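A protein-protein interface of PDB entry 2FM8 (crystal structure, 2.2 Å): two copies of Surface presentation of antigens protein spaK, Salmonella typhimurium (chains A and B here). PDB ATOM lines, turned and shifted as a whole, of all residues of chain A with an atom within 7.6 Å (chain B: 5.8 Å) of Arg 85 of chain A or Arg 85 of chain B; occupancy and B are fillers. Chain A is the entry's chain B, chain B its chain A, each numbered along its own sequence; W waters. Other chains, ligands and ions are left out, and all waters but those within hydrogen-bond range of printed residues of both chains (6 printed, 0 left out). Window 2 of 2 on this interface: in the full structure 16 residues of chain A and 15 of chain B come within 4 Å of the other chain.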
ATOM      1  N   MET A   1      -1.455  -2.498  10.433  1.00  0.00           N
ATOM      2  CA  MET A   1      -2.917  -2.815  10.583  1.00  0.00           C
ATOM      3  C   MET A   1      -3.680  -3.122   9.274  1.00  0.00           C
ATOM      4  O   MET A   1      -4.749  -3.747   9.316  1.00  0.00           O
ATOM      5  CB  MET A   1      -3.641  -1.690  11.342  1.00  0.00           C
ATOM      6  CG  MET A   1      -4.989  -2.125  11.954  1.00  0.00           C
ATOM      7  SD  MET A   1      -4.851  -3.580  13.046  1.00  0.00           S
ATOM      8  CE  MET A   1      -4.083  -2.801  14.482  1.00  0.00           C
ATOM      9  N   ASP A  49     -13.228  -3.730   9.775  1.00  0.00           N
ATOM     10  CA  ASP A  49     -12.871  -2.299   9.659  1.00  0.00           C
ATOM     11  C   ASP A  49     -11.623  -1.951  10.462  1.00  0.00           C
ATOM     12  O   ASP A  49     -11.609  -0.943  11.172  1.00  0.00           O
ATOM     13  CB  ASP A  49     -14.019  -1.379  10.155  1.00  0.00           C
ATOM     14  CG  ASP A  49     -15.276  -1.463   9.300  1.00  0.00           C
ATOM     15  OD1 ASP A  49     -16.356  -1.798   9.856  1.00  0.00           O
ATOM     16  OD2 ASP A  49     -15.190  -1.178   8.085  1.00  0.00           O
ATOM     17  N   ASP A  50     -10.591  -2.770  10.378  1.00  0.00           N
ATOM     18  CA  ASP A  50      -9.367  -2.517  11.141  1.00  0.00           C
ATOM     19  C   ASP A  50      -9.445  -2.941  12.624  1.00  0.00           C
ATOM     20  O   ASP A  50      -8.422  -2.918  13.326  1.00  0.00           O
ATOM     21  CB  ASP A  50      -8.909  -1.047  11.006  1.00  0.00           C
ATOM     22  CG  ASP A  50      -8.516  -0.673   9.543  1.00  0.00           C
ATOM     23  OD1 ASP A  50      -8.040  -1.577   8.796  1.00  0.00           O
ATOM     24  OD2 ASP A  50      -8.668   0.516   9.145  1.00  0.00           O
ATOM     25  N   ASP A  51     -10.623  -3.375  13.079  1.00  0.00           N
ATOM     26  CA  ASP A  51     -10.795  -3.889  14.436  1.00  0.00           C
ATOM     27  C   ASP A  51     -10.649  -5.414  14.490  1.00  0.00           C
ATOM     28  O   ASP A  51     -11.199  -6.116  13.649  1.00  0.00           O
ATOM     29  CB  ASP A  51     -12.184  -3.513  14.971  1.00  0.00           C
ATOM     30  CG  ASP A  51     -12.335  -2.022  15.264  1.00  0.00           C
ATOM     31  OD1 ASP A  51     -11.316  -1.373  15.575  1.00  0.00           O
ATOM     32  OD2 ASP A  51     -13.488  -1.517  15.220  1.00  0.00           O
ATOM     33  N   VAL A  52      -9.935  -5.909  15.502  1.00  0.00           N
ATOM     34  CA  VAL A  52      -9.861  -7.348  15.774  1.00  0.00           C
ATOM     35  C   VAL A  52     -10.721  -7.685  16.985  1.00  0.00           C
ATOM     36  O   VAL A  52     -10.576  -7.118  18.079  1.00  0.00           O
ATOM     37  CB  VAL A  52      -8.423  -7.823  16.017  1.00  0.00           C
ATOM     38  CG1 VAL A  52      -8.394  -9.288  16.477  1.00  0.00           C
ATOM     39  CG2 VAL A  52      -7.585  -7.628  14.742  1.00  0.00           C
ATOM     40  N   TRP A  53     -11.631  -8.612  16.748  1.00  0.00           N
ATOM     41  CA  TRP A  53     -12.558  -9.095  17.725  1.00  0.00           C
ATOM     42  C   TRP A  53     -12.258 -10.559  18.035  1.00  0.00           C
ATOM     43  O   TRP A  53     -11.888 -11.342  17.145  1.00  0.00           O
ATOM     44  CB  TRP A  53     -13.968  -9.027  17.170  1.00  0.00           C
ATOM     45  CG  TRP A  53     -14.520  -7.652  16.972  1.00  0.00           C
ATOM     46  CD1 TRP A  53     -14.493  -6.913  15.838  1.00  0.00           C
ATOM     47  CD2 TRP A  53     -15.218  -6.879  17.942  1.00  0.00           C
ATOM     48  NE1 TRP A  53     -15.141  -5.710  16.033  1.00  0.00           N
ATOM     49  CE2 TRP A  53     -15.594  -5.666  17.323  1.00  0.00           C
ATOM     50  CE3 TRP A  53     -15.579  -7.099  19.276  1.00  0.00           C
ATOM     51  CZ2 TRP A  53     -16.302  -4.678  17.991  1.00  0.00           C
ATOM     52  CZ3 TRP A  53     -16.286  -6.108  19.945  1.00  0.00           C
ATOM     53  CH2 TRP A  53     -16.652  -4.924  19.298  1.00  0.00           C
ATOM     54  N   CYS A  81     -11.144  -5.883  31.839  1.00  0.00           N
ATOM     55  CA  CYS A  81     -10.410  -6.856  31.066  1.00  0.00           C
ATOM     56  C   CYS A  81      -9.231  -6.123  30.440  1.00  0.00           C
ATOM     57  O   CYS A  81      -9.425  -5.242  29.594  1.00  0.00           O
ATOM     58  CB  CYS A  81     -11.328  -7.439  29.993  1.00  0.00           C
ATOM     59  SG  CYS A  81     -10.507  -8.458  28.750  1.00  0.00           S
ATOM     60  N   HIS A  82      -8.014  -6.476  30.864  1.00  0.00           N
ATOM     61  CA  HIS A  82      -6.814  -5.688  30.537  1.00  0.00           C
ATOM     62  C   HIS A  82      -6.498  -5.674  29.044  1.00  0.00           C
ATOM     63  O   HIS A  82      -5.902  -4.720  28.577  1.00  0.00           O
ATOM     64  CB  HIS A  82      -5.551  -6.170  31.277  1.00  0.00           C
ATOM     65  CG  HIS A  82      -5.674  -6.247  32.786  1.00  0.00           C
ATOM     66  ND1 HIS A  82      -6.381  -5.328  33.551  1.00  0.00           N
ATOM     67  CD2 HIS A  82      -5.110  -7.112  33.673  1.00  0.00           C
ATOM     68  CE1 HIS A  82      -6.269  -5.650  34.836  1.00  0.00           C
ATOM     69  NE2 HIS A  82      -5.505  -6.729  34.936  1.00  0.00           N
ATOM     70  N   PHE A  83      -6.878  -6.706  28.288  1.00  0.00           N
ATOM     71  CA  PHE A  83      -6.506  -6.767  26.859  1.00  0.00           C
ATOM     72  C   PHE A  83      -7.538  -6.166  25.892  1.00  0.00           C
ATOM     73  O   PHE A  83      -7.298  -6.124  24.702  1.00  0.00           O
ATOM     74  CB  PHE A  83      -6.137  -8.199  26.427  1.00  0.00           C
ATOM     75  CG  PHE A  83      -7.238  -9.190  26.615  1.00  0.00           C
ATOM     76  CD1 PHE A  83      -8.204  -9.361  25.644  1.00  0.00           C
ATOM     77  CD2 PHE A  83      -7.310  -9.942  27.771  1.00  0.00           C
ATOM     78  CE1 PHE A  83      -9.223 -10.268  25.820  1.00  0.00           C
ATOM     79  CE2 PHE A  83      -8.309 -10.835  27.950  1.00  0.00           C
ATOM     80  CZ  PHE A  83      -9.275 -11.007  26.963  1.00  0.00           C
ATOM     81  N   ALA A  84      -8.674  -5.694  26.403  1.00  0.00           N
ATOM     82  CA  ALA A  84      -9.705  -5.095  25.569  1.00  0.00           C
ATOM     83  C   ALA A  84      -9.525  -3.568  25.415  1.00  0.00           C
ATOM     84  O   ALA A  84      -9.086  -2.888  26.344  1.00  0.00           O
ATOM     85  CB  ALA A  84     -11.090  -5.415  26.143  1.00  0.00           C
ATOM     86  N   ARG A  85      -9.865  -3.043  24.239  1.00  0.00           N
ATOM     87  CA  ARG A  85     -10.051  -1.582  24.074  1.00  0.00           C
ATOM     88  C   ARG A  85     -11.060  -1.111  25.089  1.00  0.00           C
ATOM     89  O   ARG A  85     -12.139  -1.719  25.246  1.00  0.00           O
ATOM     90  CB  ARG A  85     -10.680  -1.257  22.743  1.00  0.00           C
ATOM     91  CG  ARG A  85      -9.797  -1.380  21.610  1.00  0.00           C
ATOM     92  CD  ARG A  85      -9.283  -0.070  21.237  1.00  0.00           C
ATOM     93  NE  ARG A  85      -8.809  -0.104  19.873  1.00  0.00           N
ATOM     94  CZ  ARG A  85      -7.978   0.786  19.369  1.00  0.00           C
ATOM     95  NH1 ARG A  85      -7.542   1.781  20.128  1.00  0.00           N
ATOM     96  NH2 ARG A  85      -7.588   0.672  18.108  1.00  0.00           N
ATOM     97  N   GLY A  86     -10.742  -0.029  25.762  1.00  0.00           N
ATOM     98  CA  GLY A  86     -11.642   0.494  26.746  1.00  0.00           C
ATOM     99  C   GLY A  86     -11.533  -0.171  28.092  1.00  0.00           C
ATOM    100  O   GLY A  86     -12.160   0.273  29.022  1.00  0.00           O
ATOM    101  N   GLY A  87     -10.747  -1.226  28.208  1.00  0.00           N
ATOM    102  CA  GLY A  87     -10.559  -1.930  29.487  1.00  0.00           C
ATOM    103  C   GLY A  87     -11.739  -2.830  29.878  1.00  0.00           C
ATOM    104  O   GLY A  87     -11.830  -3.247  31.021  1.00  0.00           O
ATOM    105  N   GLN A  88     -12.616  -3.153  28.924  1.00  0.00           N
ATOM    106  CA  GLN A  88     -13.858  -3.840  29.232  1.00  0.00           C
ATOM    107  C   GLN A  88     -14.351  -4.805  28.134  1.00  0.00           C
ATOM    108  O   GLN A  88     -14.333  -4.485  26.944  1.00  0.00           O
ATOM    109  CB  GLN A  88     -14.912  -2.795  29.525  1.00  0.00           C
ATOM    110  CG  GLN A  88     -15.930  -3.215  30.499  1.00  0.00           C
ATOM    111  CD  GLN A  88     -16.740  -2.052  31.050  1.00  0.00           C
ATOM    112  OE1 GLN A  88     -16.333  -1.392  32.002  1.00  0.00           O
ATOM    113  NE2 GLN A  88     -17.877  -1.802  30.456  1.00  0.00           N
ATOM    114  N   LEU A  89     -14.780  -6.002  28.542  1.00  0.00           N
ATOM    115  CA  LEU A  89     -15.487  -6.889  27.626  1.00  0.00           C
ATOM    116  C   LEU A  89     -16.894  -6.344  27.320  1.00  0.00           C
ATOM    117  O   LEU A  89     -17.467  -5.604  28.127  1.00  0.00           O
ATOM    118  CB  LEU A  89     -15.587  -8.271  28.220  1.00  0.00           C
ATOM    119  CG  LEU A  89     -14.254  -9.016  28.334  1.00  0.00           C
ATOM    120  CD1 LEU A  89     -14.335 -10.025  29.485  1.00  0.00           C
ATOM    121  CD2 LEU A  89     -13.928  -9.684  27.046  1.00  0.00           C
ATOM    122  N   LEU A  90     -17.424  -6.717  26.155  1.00  0.00           N
ATOM    123  CA  LEU A  90     -18.759  -6.308  25.698  1.00  0.00           C
ATOM    124  C   LEU A  90     -19.677  -7.529  25.590  1.00  0.00           C
ATOM    125  O   LEU A  90     -19.237  -8.638  25.334  1.00  0.00           O
ATOM    126  CB  LEU A  90     -18.697  -5.643  24.312  1.00  0.00           C
ATOM    127  CG  LEU A  90     -17.669  -4.529  24.140  1.00  0.00           C
ATOM    128  CD1 LEU A  90     -17.606  -4.027  22.725  1.00  0.00           C
ATOM    129  CD2 LEU A  90     -17.971  -3.386  25.091  1.00  0.00           C
ATOM    130  N   ALA A 102     -14.556  -9.290  22.888  1.00  0.00           N
ATOM    131  CA  ALA A 102     -13.418  -8.441  23.172  1.00  0.00           C
ATOM    132  C   ALA A 102     -12.994  -7.760  21.897  1.00  0.00           C
ATOM    133  O   ALA A 102     -12.671  -8.426  20.920  1.00  0.00           O
ATOM    134  CB  ALA A 102     -12.266  -9.227  23.731  1.00  0.00           C
ATOM    135  N   LEU A 103     -13.008  -6.434  21.917  1.00  0.00           N
ATOM    136  CA  LEU A 103     -12.312  -5.635  20.905  1.00  0.00           C
ATOM    137  C   LEU A 103     -10.877  -5.564  21.378  1.00  0.00           C
ATOM    138  O   LEU A 103     -10.577  -4.897  22.368  1.00  0.00           O
ATOM    139  CB  LEU A 103     -12.921  -4.240  20.787  1.00  0.00           C
ATOM    140  CG  LEU A 103     -12.325  -3.244  19.785  1.00  0.00           C
ATOM    141  CD1 LEU A 103     -12.258  -3.801  18.407  1.00  0.00           C
ATOM    142  CD2 LEU A 103     -13.132  -1.957  19.754  1.00  0.00           C
ATOM    143  N   VAL A 104      -9.999  -6.265  20.674  1.00  0.00           N
ATOM    144  CA  VAL A 104      -8.625  -6.430  21.119  1.00  0.00           C
ATOM    145  C   VAL A 104      -7.828  -5.135  20.970  1.00  0.00           C
ATOM    146  O   VAL A 104      -7.747  -4.530  19.875  1.00  0.00           O
ATOM    147  CB  VAL A 104      -7.918  -7.629  20.416  1.00  0.00           C
ATOM    148  CG1 VAL A 104      -6.507  -7.809  20.950  1.00  0.00           C
ATOM    149  CG2 VAL A 104      -8.704  -8.909  20.667  1.00  0.00           C
ATOM    150  N   HIS A 105      -7.242  -4.713  22.091  1.00  0.00           N
ATOM    151  CA  HIS A 105      -6.355  -3.558  22.084  1.00  0.00           C
ATOM    152  C   HIS A 105      -5.110  -3.825  21.207  1.00  0.00           C
ATOM    153  O   HIS A 105      -4.542  -4.927  21.237  1.00  0.00           O
ATOM    154  CB  HIS A 105      -5.956  -3.137  23.501  1.00  0.00           C
ATOM    155  CG  HIS A 105      -5.303  -1.783  23.539  1.00  0.00           C
ATOM    156  ND1 HIS A 105      -3.997  -1.578  23.145  1.00  0.00           N
ATOM    157  CD2 HIS A 105      -5.800  -0.562  23.839  1.00  0.00           C
ATOM    158  CE1 HIS A 105      -3.708  -0.294  23.228  1.00  0.00           C
ATOM    159  NE2 HIS A 105      -4.790   0.346  23.642  1.00  0.00           N
ATOM    160  N   PRO A 106      -4.705  -2.826  20.392  1.00  0.00           N
ATOM    161  CA  PRO A 106      -3.562  -2.994  19.490  1.00  0.00           C
ATOM    162  C   PRO A 106      -2.248  -3.428  20.149  1.00  0.00           C
ATOM    163  O   PRO A 106      -1.437  -4.058  19.496  1.00  0.00           O
ATOM    164  CB  PRO A 106      -3.415  -1.609  18.841  1.00  0.00           C
ATOM    165  CG  PRO A 106      -4.747  -0.991  18.971  1.00  0.00           C
ATOM    166  CD  PRO A 106      -5.322  -1.491  20.243  1.00  0.00           C
ATOM    167  N   ASP A 107      -2.046  -3.111  21.422  1.00  0.00           N
ATOM    168  CA  ASP A 107      -0.908  -3.639  22.184  1.00  0.00           C
ATOM    169  C   ASP A 107      -0.842  -5.146  22.224  1.00  0.00           C
ATOM    170  O   ASP A 107       0.227  -5.709  22.443  1.00  0.00           O
ATOM    171  CB  ASP A 107      -0.915  -3.126  23.630  1.00  0.00           C
ATOM    172  CG  ASP A 107      -0.666  -1.636  23.710  1.00  0.00           C
ATOM    173  OD1 ASP A 107      -0.329  -1.034  22.675  1.00  0.00           O
ATOM    174  OD2 ASP A 107      -0.824  -1.058  24.800  1.00  0.00           O
ATOM    175  N   PHE A 108      -1.966  -5.810  21.995  1.00  0.00           N
ATOM    176  CA  PHE A 108      -1.984  -7.264  21.981  1.00  0.00           C
ATOM    177  C   PHE A 108      -2.048  -7.848  20.584  1.00  0.00           C
ATOM    178  O   PHE A 108      -2.304  -9.037  20.420  1.00  0.00           O
ATOM    179  CB  PHE A 108      -3.126  -7.748  22.873  1.00  0.00           C
ATOM    180  CG  PHE A 108      -2.896  -7.462  24.317  1.00  0.00           C
ATOM    181  CD1 PHE A 108      -2.251  -8.386  25.113  1.00  0.00           C
ATOM    182  CD2 PHE A 108      -3.284  -6.258  24.869  1.00  0.00           C
ATOM    183  CE1 PHE A 108      -2.004  -8.122  26.459  1.00  0.00           C
ATOM    184  CE2 PHE A 108      -3.032  -5.974  26.207  1.00  0.00           C
ATOM    185  CZ  PHE A 108      -2.399  -6.916  27.009  1.00  0.00           C
ATOM    186  N   LEU A 109      -1.780  -7.024  19.576  1.00  0.00           N
ATOM    187  CA  LEU A 109      -1.797  -7.485  18.191  1.00  0.00           C
ATOM    188  C   LEU A 109      -0.412  -7.422  17.532  1.00  0.00           C
ATOM    189  O   LEU A 109      -0.297  -7.672  16.337  1.00  0.00           O
ATOM    190  CB  LEU A 109      -2.783  -6.645  17.374  1.00  0.00           C
ATOM    191  CG  LEU A 109      -4.236  -6.594  17.840  1.00  0.00           C
ATOM    192  CD1 LEU A 109      -5.024  -5.561  17.013  1.00  0.00           C
ATOM    193  CD2 LEU A 109      -4.873  -7.960  17.731  1.00  0.00           C
ATOM    194  N   MET B   1      -4.362  12.631  14.982  1.00  0.00           N
ATOM    195  CA  MET B   1      -4.616  11.895  16.282  1.00  0.00           C
ATOM    196  C   MET B   1      -3.557  12.263  17.322  1.00  0.00           C
ATOM    197  O   MET B   1      -3.445  11.636  18.379  1.00  0.00           O
ATOM    198  CB  MET B   1      -4.627  10.372  16.050  1.00  0.00           C
ATOM    199  CG  MET B   1      -5.422   9.536  17.084  1.00  0.00           C
ATOM    200  SD  MET B   1      -7.231   9.818  17.212  1.00  0.00           S
ATOM    201  CE  MET B   1      -7.666  10.360  15.566  1.00  0.00           C
ATOM    202  N   ASP B  51      -6.495   8.548  23.312  1.00  0.00           N
ATOM    203  CA  ASP B  51      -7.893   8.136  23.282  1.00  0.00           C
ATOM    204  C   ASP B  51      -8.724   9.335  23.733  1.00  0.00           C
ATOM    205  O   ASP B  51      -8.409   9.955  24.735  1.00  0.00           O
ATOM    206  CB  ASP B  51      -8.158   6.997  24.263  1.00  0.00           C
ATOM    207  CG  ASP B  51      -7.428   5.706  23.909  1.00  0.00           C
ATOM    208  OD1 ASP B  51      -7.428   5.315  22.735  1.00  0.00           O
ATOM    209  OD2 ASP B  51      -6.891   5.060  24.829  1.00  0.00           O
ATOM    210  N   CYS B  81     -24.055   1.975  20.165  1.00  0.00           N
ATOM    211  CA  CYS B  81     -23.689   3.376  20.115  1.00  0.00           C
ATOM    212  C   CYS B  81     -22.756   3.553  18.922  1.00  0.00           C
ATOM    213  O   CYS B  81     -21.611   3.073  18.938  1.00  0.00           O
ATOM    214  CB  CYS B  81     -23.008   3.786  21.401  1.00  0.00           C
ATOM    215  SG  CYS B  81     -22.431   5.448  21.374  1.00  0.00           S
ATOM    216  N   PHE B  83     -21.029   5.955  17.691  1.00  0.00           N
ATOM    217  CA  PHE B  83     -19.825   6.821  17.742  1.00  0.00           C
ATOM    218  C   PHE B  83     -18.730   6.308  18.703  1.00  0.00           C
ATOM    219  O   PHE B  83     -17.664   6.924  18.845  1.00  0.00           O
ATOM    220  CB  PHE B  83     -20.188   8.302  18.025  1.00  0.00           C
ATOM    221  CG  PHE B  83     -20.942   8.510  19.309  1.00  0.00           C
ATOM    222  CD1 PHE B  83     -20.272   8.583  20.519  1.00  0.00           C
ATOM    223  CD2 PHE B  83     -22.325   8.595  19.312  1.00  0.00           C
ATOM    224  CE1 PHE B  83     -20.975   8.742  21.712  1.00  0.00           C
ATOM    225  CE2 PHE B  83     -23.026   8.748  20.504  1.00  0.00           C
ATOM    226  CZ  PHE B  83     -22.350   8.829  21.695  1.00  0.00           C
ATOM    227  N   ALA B  84     -18.988   5.168  19.327  1.00  0.00           N
ATOM    228  CA  ALA B  84     -18.061   4.561  20.257  1.00  0.00           C
ATOM    229  C   ALA B  84     -17.258   3.447  19.578  1.00  0.00           C
ATOM    230  O   ALA B  84     -17.764   2.710  18.715  1.00  0.00           O
ATOM    231  CB  ALA B  84     -18.806   4.002  21.465  1.00  0.00           C
ATOM    232  N   ARG B  85     -16.004   3.329  19.985  1.00  0.00           N
ATOM    233  CA  ARG B  85     -15.199   2.189  19.599  1.00  0.00           C
ATOM    234  C   ARG B  85     -15.882   0.956  20.123  1.00  0.00           C
ATOM    235  O   ARG B  85     -16.324   0.952  21.242  1.00  0.00           O
ATOM    236  CB  ARG B  85     -13.828   2.255  20.236  1.00  0.00           C
ATOM    237  CG  ARG B  85     -12.888   3.074  19.516  1.00  0.00           C
ATOM    238  CD  ARG B  85     -11.522   2.609  19.839  1.00  0.00           C
ATOM    239  NE  ARG B  85     -10.511   3.548  19.357  1.00  0.00           N
ATOM    240  CZ  ARG B  85      -9.937   3.498  18.155  1.00  0.00           C
ATOM    241  NH1 ARG B  85     -10.290   2.585  17.256  1.00  0.00           N
ATOM    242  NH2 ARG B  85      -9.013   4.397  17.844  1.00  0.00           N
ATOM    243  N   GLY B  86     -15.988  -0.074  19.305  1.00  0.00           N
ATOM    244  CA  GLY B  86     -16.665  -1.295  19.710  1.00  0.00           C
ATOM    245  C   GLY B  86     -18.172  -1.234  19.564  1.00  0.00           C
ATOM    246  O   GLY B  86     -18.840  -2.232  19.799  1.00  0.00           O
ATOM    247  N   GLY B  87     -18.708  -0.078  19.176  1.00  0.00           N
ATOM    248  CA  GLY B  87     -20.146   0.065  18.953  1.00  0.00           C
ATOM    249  C   GLY B  87     -20.985   0.056  20.223  1.00  0.00           C
ATOM    250  O   GLY B  87     -22.187  -0.184  20.171  1.00  0.00           O
ATOM    251  N   GLN B  88     -20.351   0.364  21.357  1.00  0.00           N
ATOM    252  CA  GLN B  88     -20.992   0.248  22.628  1.00  0.00           C
ATOM    253  C   GLN B  88     -20.441   1.198  23.696  1.00  0.00           C
ATOM    254  O   GLN B  88     -19.233   1.343  23.854  1.00  0.00           O
ATOM    255  CB  GLN B  88     -20.876  -1.213  23.109  1.00  0.00           C
ATOM    256  CG  GLN B  88     -22.126  -1.736  23.682  1.00  0.00           C
ATOM    257  CD  GLN B  88     -22.095  -3.230  23.953  1.00  0.00           C
ATOM    258  OE1 GLN B  88     -22.672  -4.023  23.198  1.00  0.00           O
ATOM    259  NE2 GLN B  88     -21.474  -3.615  25.065  1.00  0.00           N
ATOM    260  N   LEU B  90     -19.694   2.132  27.636  1.00  0.00           N
ATOM    261  CA  LEU B  90     -19.094   1.349  28.732  1.00  0.00           C
ATOM    262  C   LEU B  90     -19.584   1.931  30.042  1.00  0.00           C
ATOM    263  O   LEU B  90     -19.936   3.101  30.125  1.00  0.00           O
ATOM    264  CB  LEU B  90     -17.546   1.429  28.704  1.00  0.00           C
ATOM    265  CG  LEU B  90     -16.875   0.966  27.411  1.00  0.00           C
ATOM    266  CD1 LEU B  90     -15.378   1.104  27.457  1.00  0.00           C
ATOM    267  CD2 LEU B  90     -17.221  -0.484  27.075  1.00  0.00           C
ATOM    268  N   LEU B 103     -15.647   5.665  24.599  1.00  0.00           N
ATOM    269  CA  LEU B 103     -14.353   5.759  23.971  1.00  0.00           C
ATOM    270  C   LEU B 103     -14.665   6.103  22.541  1.00  0.00           C
ATOM    271  O   LEU B 103     -15.093   5.267  21.779  1.00  0.00           O
ATOM    272  CB  LEU B 103     -13.595   4.421  24.060  1.00  0.00           C
ATOM    273  CG  LEU B 103     -12.250   4.340  23.332  1.00  0.00           C
ATOM    274  CD1 LEU B 103     -11.316   5.381  23.868  1.00  0.00           C
ATOM    275  CD2 LEU B 103     -11.645   2.965  23.474  1.00  0.00           C
ATOM    276  N   VAL B 104     -14.462   7.356  22.177  1.00  0.00           N
ATOM    277  CA  VAL B 104     -14.923   7.855  20.889  1.00  0.00           C
ATOM    278  C   VAL B 104     -14.123   7.280  19.708  1.00  0.00           C
ATOM    279  O   VAL B 104     -12.890   7.314  19.706  1.00  0.00           O
ATOM    280  CB  VAL B 104     -14.829   9.368  20.811  1.00  0.00           C
ATOM    281  CG1 VAL B 104     -15.424   9.864  19.505  1.00  0.00           C
ATOM    282  CG2 VAL B 104     -15.540  10.026  22.007  1.00  0.00           C
ATOM    283  N   HIS B 105     -14.840   6.809  18.693  1.00  0.00           N
ATOM    284  CA  HIS B 105     -14.200   6.289  17.505  1.00  0.00           C
ATOM    285  C   HIS B 105     -13.567   7.469  16.744  1.00  0.00           C
ATOM    286  O   HIS B 105     -14.177   8.514  16.660  1.00  0.00           O
ATOM    287  CB  HIS B 105     -15.227   5.554  16.639  1.00  0.00           C
ATOM    288  CG  HIS B 105     -14.613   4.763  15.520  1.00  0.00           C
ATOM    289  ND1 HIS B 105     -14.025   5.358  14.426  1.00  0.00           N
ATOM    290  CD2 HIS B 105     -14.471   3.427  15.344  1.00  0.00           C
ATOM    291  CE1 HIS B 105     -13.560   4.420  13.615  1.00  0.00           C
ATOM    292  NE2 HIS B 105     -13.814   3.240  14.151  1.00  0.00           N
ATOM    293  N   PRO B 106     -12.329   7.317  16.221  1.00  0.00           N
ATOM    294  CA  PRO B 106     -11.693   8.409  15.459  1.00  0.00           C
ATOM    295  C   PRO B 106     -12.475   8.977  14.259  1.00  0.00           C
ATOM    296  O   PRO B 106     -12.297  10.135  13.926  1.00  0.00           O
ATOM    297  CB  PRO B 106     -10.358   7.799  15.003  1.00  0.00           C
ATOM    298  CG  PRO B 106     -10.113   6.682  15.916  1.00  0.00           C
ATOM    299  CD  PRO B 106     -11.439   6.153  16.346  1.00  0.00           C
HETATM  300  O   HOH W   1      -8.088   2.290  22.819  1.00  0.00           O
HETATM  301  O   HOH W   2     -12.429   0.798  17.256  1.00  0.00           O
HETATM  302  O   HOH W   3      -4.843   3.109  24.770  1.00  0.00           O
HETATM  303  O   HOH W   4     -11.172   2.074  12.185  1.00  0.00           O
HETATM  304  O   HOH W   5     -14.954   0.321  16.720  1.00  0.00           O
HETATM  305  O   HOH W   6     -13.454   0.489  13.119  1.00  0.00           O
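The guanidinium group (NH2) of Arg 85 of chain A sits close to the guanidinium group (NH1) of Arg 85 of chain B.
N of Arg 85 of chain B lies within hydrogen-bond range of O of Leu 103 of chain B. N of Arg 85 of chain A lies within hydrogen-bond range of O of Leu 103 of chain A, 2.7 Å away.
Among the printed residues, merely in contact across the chains: Leu 103 of chain A with Gly 86 of chain B (3.5 Å), Trp 53 of chain A with Gly 86 of chain B (3.5 Å), Leu 90 of chain A with Gln 88 of chain B (3.5 Å), Leu 90 of chain A with Leu 90 of chain B (3.6 Å), Leu 90 of chain A with Gly 86 of chain B (3.6 Å), Gly 86 of chain A with Leu 90 of chain B (3.7 Å), Gln 88 of chain A with Leu 90 of chain B (3.7 Å) and Gly 86 of chain A with Leu 103 of chain B (3.9 Å).
Asp 50 of chain A touches none of the printed residues of chain B. Printed residues of chain B within 4 Å of Trp 53 of chain A: Gly 86 (3.5 Å). Of chain B, only Arg 85 (3.4 Å) comes within 4 Å of Arg 85 of chain A. Printed residues of chain B within 4 Å of Gly 86 of chain A: Leu 90 and Leu 103. Gly 87 of chain A touches none of the printed residues of chain B. Of chain A, only Arg 85 (3.4 Å) comes within 4 Å of Arg 85 of chain B. Of the printed residues of chain A, Gln 88 of chain B touches Leu 90 (3.5 Å). Printed residues of chain A within 4 Å of Leu 90 of chain B: Gly 86 (3.7 Å), Gln 88 (3.7 Å) and Leu 90 (3.6 Å). The nearest printed residue of chain B that does not touch Arg 85 of chain A is Leu 103 of chain B (4.4 Å). The nearest residue of chain A that does not touch Arg 85 of chain B is Leu 103 of chain A (4.02 Å). The nearest printed residue of chain B that does not touch Gln 88 of chain A is Gln 88 of chain B (6.7 Å).
Of the 14 printed residues of chain B, 5 touch a printed residue of chain A. Printed residues of chain B that touch a printed residue of chain A: Arg 85, Gly 86, Gln 88, Leu 90 and Leu 103. Hydrophobic or aromatic side chains of chain A that line the printed part of chain B: Trp 53, Leu 90 and Leu 103. Among the printed residues, 9 pairs touch across the chains. Among the printed residues, no Asp or Glu carboxylate lies within 4 Å of a Lys or Arg side-chain nitrogen of the other chain.
Gly 86 of chain A touches Leu 90 of chain B, and with the chains exchanged Leu 90 of chain A touches Gly 86 of chain B. Gly 86 of chain A touches Leu 103 of chain B, and with the chains exchanged Leu 103 of chain A touches Gly 86 of chain B. Gln 88 of chain A touches Leu 90 of chain B, and with the chains exchanged Leu 90 of chain A touches Gln 88 of chain B. Leu 90 of chain B touches its own counterpart, Leu 90 of chain A. Positions printed for both chains: 1, 51, 81, 83, 84, 85, 86, 87, 88, 90, 103, 104, 105 and 106.
Water W2 lies within hydrogen-bond range of the guanidinium group of Arg 85 of chain B and the side-chain carboxylate of Asp 51 of chain A. Water W1 lies within hydrogen-bond range of NH1 of Arg 85 of chain A (2.8 Å) and OD1 of Asp 51 of chain B (3.1 Å). Water W6 lies within hydrogen-bond range of OD2 of Asp 51 of chain A (2.9 Å), NE2 of His 105 of chain B (3.0 Å) and O of Asp 49 of chain A (3.0 Å). Water W4 lies within hydrogen-bond range of O of Asp 49 of chain A and NE2 of His 105 of chain B.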
